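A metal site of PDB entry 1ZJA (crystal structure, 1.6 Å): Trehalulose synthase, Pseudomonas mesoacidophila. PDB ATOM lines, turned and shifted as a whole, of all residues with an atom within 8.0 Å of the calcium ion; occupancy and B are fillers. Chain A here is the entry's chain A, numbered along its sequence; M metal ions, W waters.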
ATOM      1  N   PRO A  17       4.601 -15.582 -28.291  1.00  0.00           N
ATOM      2  CA  PRO A  17       4.715 -16.941 -27.723  1.00  0.00           C
ATOM      3  C   PRO A  17       5.909 -17.788 -28.088  1.00  0.00           C
ATOM      4  O   PRO A  17       6.478 -18.472 -27.238  1.00  0.00           O
ATOM      5  CB  PRO A  17       3.380 -17.602 -28.098  1.00  0.00           C
ATOM      6  CG  PRO A  17       2.424 -16.437 -28.275  1.00  0.00           C
ATOM      7  CD  PRO A  17       3.303 -15.430 -28.989  1.00  0.00           C
ATOM      8  N   ARG A  18       6.280 -17.735 -29.349  1.00  0.00           N
ATOM      9  CA  ARG A  18       7.400 -18.486 -29.883  1.00  0.00           C
ATOM     10  C   ARG A  18       8.703 -18.265 -29.101  1.00  0.00           C
ATOM     11  O   ARG A  18       9.548 -19.170 -29.021  1.00  0.00           O
ATOM     12  CB  ARG A  18       7.597 -18.063 -31.345  1.00  0.00           C
ATOM     13  CG  ARG A  18       8.594 -18.859 -32.095  1.00  0.00           C
ATOM     14  CD  ARG A  18       8.618 -18.387 -33.563  1.00  0.00           C
ATOM     15  NE  ARG A  18       9.559 -19.232 -34.269  1.00  0.00           N
ATOM     16  CZ  ARG A  18       9.262 -20.428 -34.774  1.00  0.00           C
ATOM     17  NH1 ARG A  18       8.029 -20.943 -34.682  1.00  0.00           N
ATOM     18  NH2 ARG A  18      10.233 -21.147 -35.330  1.00  0.00           N
ATOM     19  N   LYS A  21       8.318 -18.565 -23.340  1.00  0.00           N
ATOM     20  CA  LYS A  21       8.756 -19.646 -22.436  1.00  0.00           C
ATOM     21  C   LYS A  21       8.442 -21.032 -23.003  1.00  0.00           C
ATOM     22  O   LYS A  21       7.283 -21.324 -23.319  1.00  0.00           O
ATOM     23  CB  LYS A  21       8.097 -19.502 -21.057  1.00  0.00           C
ATOM     24  CG  LYS A  21       8.530 -20.586 -20.061  1.00  0.00           C
ATOM     25  CD  LYS A  21      10.029 -20.510 -19.758  1.00  0.00           C
ATOM     26  CE  LYS A  21      10.371 -21.327 -18.519  1.00  0.00           C
ATOM     27  NZ  LYS A  21       9.807 -22.685 -18.629  1.00  0.00           N
ATOM     28  N   ASP A  22       9.469 -21.865 -23.147  1.00  0.00           N
ATOM     29  CA  ASP A  22       9.319 -23.236 -23.651  1.00  0.00           C
ATOM     30  C   ASP A  22       9.142 -24.168 -22.430  1.00  0.00           C
ATOM     31  O   ASP A  22       9.807 -23.975 -21.419  1.00  0.00           O
ATOM     32  CB  ASP A  22      10.595 -23.648 -24.418  1.00  0.00           C
ATOM     33  CG  ASP A  22      10.526 -25.083 -24.985  1.00  0.00           C
ATOM     34  OD1 ASP A  22       9.451 -25.681 -25.058  1.00  0.00           O
ATOM     35  OD2 ASP A  22      11.583 -25.598 -25.409  1.00  0.00           O
ATOM     36  N   THR A  23       8.250 -25.143 -22.530  1.00  0.00           N
ATOM     37  CA  THR A  23       8.032 -26.075 -21.408  1.00  0.00           C
ATOM     38  C   THR A  23       8.232 -27.527 -21.762  1.00  0.00           C
ATOM     39  O   THR A  23       8.043 -28.400 -20.917  1.00  0.00           O
ATOM     40  CB  THR A  23       6.600 -25.926 -20.771  1.00  0.00           C
ATOM     41  OG1 THR A  23       5.611 -26.053 -21.813  1.00  0.00           O
ATOM     42  CG2 THR A  23       6.485 -24.575 -20.024  1.00  0.00           C
ATOM     43  N   ASN A  24       8.587 -27.821 -23.008  1.00  0.00           N
ATOM     44  CA  ASN A  24       8.787 -29.196 -23.375  1.00  0.00           C
ATOM     45  C   ASN A  24      10.091 -29.489 -24.107  1.00  0.00           C
ATOM     46  O   ASN A  24      10.203 -30.531 -24.732  1.00  0.00           O
ATOM     47  CB  ASN A  24       7.575 -29.709 -24.169  1.00  0.00           C
ATOM     48  CG  ASN A  24       7.510 -29.141 -25.578  1.00  0.00           C
ATOM     49  OD1 ASN A  24       8.134 -28.130 -25.891  1.00  0.00           O
ATOM     50  ND2 ASN A  24       6.731 -29.786 -26.425  1.00  0.00           N
ATOM     51  N   GLY A  25      11.055 -28.567 -24.045  1.00  0.00           N
ATOM     52  CA  GLY A  25      12.346 -28.774 -24.675  1.00  0.00           C
ATOM     53  C   GLY A  25      12.528 -28.790 -26.183  1.00  0.00           C
ATOM     54  O   GLY A  25      13.582 -29.236 -26.684  1.00  0.00           O
ATOM     55  N   ASP A  26      11.546 -28.308 -26.924  1.00  0.00           N
ATOM     56  CA  ASP A  26      11.701 -28.325 -28.358  1.00  0.00           C
ATOM     57  C   ASP A  26      12.276 -27.012 -28.856  1.00  0.00           C
ATOM     58  O   ASP A  26      12.461 -26.841 -30.055  1.00  0.00           O
ATOM     59  CB  ASP A  26      10.361 -28.649 -29.028  1.00  0.00           C
ATOM     60  CG  ASP A  26       9.374 -27.497 -28.969  1.00  0.00           C
ATOM     61  OD1 ASP A  26       9.470 -26.622 -28.089  1.00  0.00           O
ATOM     62  OD2 ASP A  26       8.475 -27.505 -29.827  1.00  0.00           O
ATOM     63  N   GLY A  27      12.608 -26.124 -27.910  1.00  0.00           N
ATOM     64  CA  GLY A  27      13.209 -24.834 -28.219  1.00  0.00           C
ATOM     65  C   GLY A  27      12.234 -23.756 -28.702  1.00  0.00           C
ATOM     66  O   GLY A  27      12.666 -22.694 -29.123  1.00  0.00           O
ATOM     67  N   ILE A  28      10.933 -24.053 -28.628  1.00  0.00           N
ATOM     68  CA  ILE A  28       9.924 -23.076 -29.049  1.00  0.00           C
ATOM     69  C   ILE A  28       8.997 -22.845 -27.867  1.00  0.00           C
ATOM     70  O   ILE A  28       8.600 -23.787 -27.175  1.00  0.00           O
ATOM     71  CB  ILE A  28       9.125 -23.574 -30.293  1.00  0.00           C
ATOM     72  CG1 ILE A  28      10.070 -23.588 -31.510  1.00  0.00           C
ATOM     73  CG2 ILE A  28       7.934 -22.642 -30.587  1.00  0.00           C
ATOM     74  CD1 ILE A  28       9.546 -24.349 -32.752  1.00  0.00           C
ATOM     75  N   GLY A  29       8.673 -21.580 -27.617  1.00  0.00           N
ATOM     76  CA  GLY A  29       7.800 -21.259 -26.500  1.00  0.00           C
ATOM     77  C   GLY A  29       6.398 -21.733 -26.777  1.00  0.00           C
ATOM     78  O   GLY A  29       6.001 -21.922 -27.921  1.00  0.00           O
ATOM     79  N   ASP A  30       5.610 -21.858 -25.707  1.00  0.00           N
ATOM     80  CA  ASP A  30       4.295 -22.442 -25.871  1.00  0.00           C
ATOM     81  C   ASP A  30       3.294 -21.888 -24.877  1.00  0.00           C
ATOM     82  O   ASP A  30       3.659 -21.118 -24.001  1.00  0.00           O
ATOM     83  CB  ASP A  30       4.421 -23.960 -25.720  1.00  0.00           C
ATOM     84  CG  ASP A  30       5.345 -24.358 -24.576  1.00  0.00           C
ATOM     85  OD1 ASP A  30       5.007 -24.080 -23.407  1.00  0.00           O
ATOM     86  OD2 ASP A  30       6.418 -24.932 -24.840  1.00  0.00           O
ATOM     87  N   PHE A  31       2.044 -22.320 -24.991  1.00  0.00           N
ATOM     88  CA  PHE A  31       1.003 -21.822 -24.110  1.00  0.00           C
ATOM     89  C   PHE A  31       1.220 -22.204 -22.660  1.00  0.00           C
ATOM     90  O   PHE A  31       0.924 -21.403 -21.778  1.00  0.00           O
ATOM     91  CB  PHE A  31      -0.346 -22.381 -24.533  1.00  0.00           C
ATOM     92  CG  PHE A  31      -0.888 -21.791 -25.777  1.00  0.00           C
ATOM     93  CD1 PHE A  31      -1.014 -20.422 -25.920  1.00  0.00           C
ATOM     94  CD2 PHE A  31      -1.395 -22.625 -26.759  1.00  0.00           C
ATOM     95  CE1 PHE A  31      -1.660 -19.887 -27.035  1.00  0.00           C
ATOM     96  CE2 PHE A  31      -2.035 -22.100 -27.866  1.00  0.00           C
ATOM     97  CZ  PHE A  31      -2.168 -20.741 -27.991  1.00  0.00           C
ATOM     98  N   LYS A  32       1.685 -23.424 -22.427  1.00  0.00           N
ATOM     99  CA  LYS A  32       1.945 -23.811 -21.034  1.00  0.00           C
ATOM    100  C   LYS A  32       3.013 -22.885 -20.433  1.00  0.00           C
ATOM    101  O   LYS A  32       2.937 -22.498 -19.261  1.00  0.00           O
ATOM    102  CB  LYS A  32       2.377 -25.280 -20.957  1.00  0.00           C
ATOM    103  CG  LYS A  32       1.228 -26.248 -21.201  1.00  0.00           C
ATOM    104  CD  LYS A  32       1.636 -27.699 -20.933  1.00  0.00           C
ATOM    105  CE  LYS A  32       0.508 -28.668 -21.302  1.00  0.00           C
ATOM    106  NZ  LYS A  32       0.975 -30.089 -21.135  1.00  0.00           N
ATOM    107  N   GLY A  33       4.025 -22.523 -21.252  1.00  0.00           N
ATOM    108  CA  GLY A  33       5.054 -21.619 -20.746  1.00  0.00           C
ATOM    109  C   GLY A  33       4.459 -20.279 -20.346  1.00  0.00           C
ATOM    110  O   GLY A  33       4.757 -19.741 -19.281  1.00  0.00           O
ATOM    111  N   LYS A  74       0.198 -26.053 -33.528  1.00  0.00           N
ATOM    112  CA  LYS A  74       0.690 -27.302 -32.903  1.00  0.00           C
ATOM    113  C   LYS A  74       1.840 -27.066 -31.920  1.00  0.00           C
ATOM    114  O   LYS A  74       1.872 -27.643 -30.820  1.00  0.00           O
ATOM    115  CB  LYS A  74       1.108 -28.271 -33.998  1.00  0.00           C
ATOM    116  N   GLU A  75       2.777 -26.185 -32.307  1.00  0.00           N
ATOM    117  CA  GLU A  75       3.924 -25.875 -31.462  1.00  0.00           C
ATOM    118  C   GLU A  75       3.553 -25.247 -30.129  1.00  0.00           C
ATOM    119  O   GLU A  75       4.295 -25.394 -29.171  1.00  0.00           O
ATOM    120  CB  GLU A  75       4.892 -24.895 -32.178  1.00  0.00           C
ATOM    121  CG  GLU A  75       5.788 -25.478 -33.274  1.00  0.00           C
ATOM    122  CD  GLU A  75       5.042 -25.719 -34.566  1.00  0.00           C
ATOM    123  OE1 GLU A  75       3.864 -25.329 -34.686  1.00  0.00           O
ATOM    124  OE2 GLU A  75       5.631 -26.303 -35.494  1.00  0.00           O
ATOM    125  N   TYR A  76       2.428 -24.533 -30.056  1.00  0.00           N
ATOM    126  CA  TYR A  76       2.068 -23.876 -28.800  1.00  0.00           C
ATOM    127  C   TYR A  76       1.260 -24.759 -27.837  1.00  0.00           C
ATOM    128  O   TYR A  76       1.253 -24.523 -26.622  1.00  0.00           O
ATOM    129  CB  TYR A  76       1.282 -22.577 -29.062  1.00  0.00           C
ATOM    130  CG  TYR A  76       2.081 -21.517 -29.799  1.00  0.00           C
ATOM    131  CD1 TYR A  76       3.444 -21.658 -30.008  1.00  0.00           C
ATOM    132  CD2 TYR A  76       1.435 -20.387 -30.358  1.00  0.00           C
ATOM    133  CE1 TYR A  76       4.166 -20.715 -30.776  1.00  0.00           C
ATOM    134  CE2 TYR A  76       2.152 -19.438 -31.113  1.00  0.00           C
ATOM    135  CZ  TYR A  76       3.514 -19.617 -31.320  1.00  0.00           C
ATOM    136  OH  TYR A  76       4.214 -18.729 -32.119  1.00  0.00           O
ATOM    137  N   GLY A  77       0.570 -25.741 -28.407  1.00  0.00           N
ATOM    138  CA  GLY A  77      -0.207 -26.643 -27.565  1.00  0.00           C
ATOM    139  C   GLY A  77      -1.517 -27.017 -28.206  1.00  0.00           C
ATOM    140  O   GLY A  77      -1.622 -27.114 -29.434  1.00  0.00           O
ATOM    141  N   PHE A 431      15.015 -20.177 -20.766  1.00  0.00           N
ATOM    142  CA  PHE A 431      13.920 -20.183 -21.742  1.00  0.00           C
ATOM    143  C   PHE A 431      13.556 -21.601 -22.137  1.00  0.00           C
ATOM    144  O   PHE A 431      12.389 -21.928 -22.348  1.00  0.00           O
ATOM    145  CB  PHE A 431      14.341 -19.426 -22.991  1.00  0.00           C
ATOM    146  CG  PHE A 431      13.453 -19.676 -24.192  1.00  0.00           C
ATOM    147  CD1 PHE A 431      12.135 -19.207 -24.221  1.00  0.00           C
ATOM    148  CD2 PHE A 431      13.913 -20.417 -25.259  1.00  0.00           C
ATOM    149  CE1 PHE A 431      11.318 -19.487 -25.322  1.00  0.00           C
ATOM    150  CE2 PHE A 431      13.097 -20.697 -26.360  1.00  0.00           C
ATOM    151  CZ  PHE A 431      11.793 -20.233 -26.380  1.00  0.00           C
ATOM    152  N   THR A 432      14.572 -22.453 -22.285  1.00  0.00           N
ATOM    153  CA  THR A 432      14.322 -23.825 -22.710  1.00  0.00           C
ATOM    154  C   THR A 432      15.372 -24.770 -22.130  1.00  0.00           C
ATOM    155  O   THR A 432      16.436 -24.321 -21.720  1.00  0.00           O
ATOM    156  CB  THR A 432      14.354 -23.879 -24.256  1.00  0.00           C
ATOM    157  OG1 THR A 432      14.068 -25.191 -24.716  1.00  0.00           O
ATOM    158  CG2 THR A 432      15.735 -23.437 -24.798  1.00  0.00           C
HETATM  159 CA    CA M   1       7.694 -25.870 -26.631  1.00  0.00          CA
HETATM  160  O   HOH W   1       6.721 -25.655 -29.047  1.00  0.00           O
HETATM  161  O   HOH W   2       5.528 -26.995 -26.677  1.00  0.00           O
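The side-chain carboxylate of Asp 22 lies within hydrogen-bond range of the backbone NH of Gly 25 (3.3 Å).
N of Gly 27 sits at hydrogen-bond distance from OD2 of Asp 22, at 2.8 Å.
OG1 of Thr 432 lies within hydrogen-bond range of OD2 of Asp 22 (2.6 Å).
The backbone NH (N) of Asp 22 sits at hydrogen-bond distance from the backbone carbonyl oxygen (O) of Phe 431, at 3.0 Å.
OG1 of Thr 23 sits at hydrogen-bond distance from OD1 of Asp 30 (2.6 Å).
O of Lys 21 sits at hydrogen-bond distance from N of Asp 30 (3.0 Å).
The side-chain carboxylate (OD1) of Asp 30 sits at hydrogen-bond distance from the backbone NH (N) of Gly 33, at 2.8 Å.
The nearest printed residue that does not touch the calcium ion is Thr 23 (4.2 Å).
The calcium ion is bound by O of Ile 28 (2.3 Å), OD1 of Asp 22 (2.4 Å), OD2 of Asp 30 (2.4 Å), OD1 of Asp 26 (2.4 Å), OD1 of Asn 24 (2.4 Å), water W2 (2.4 Å) and water W1 (2.6 Å).
Water W2 lies within hydrogen-bond range of the side-chain amide nitrogen of Asn 24 and the backbone carbonyl oxygen of Glu 75.
Water W1 bridges O of Glu 75 (2.4 Å) and OD2 of Asp 26 (2.7 Å).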
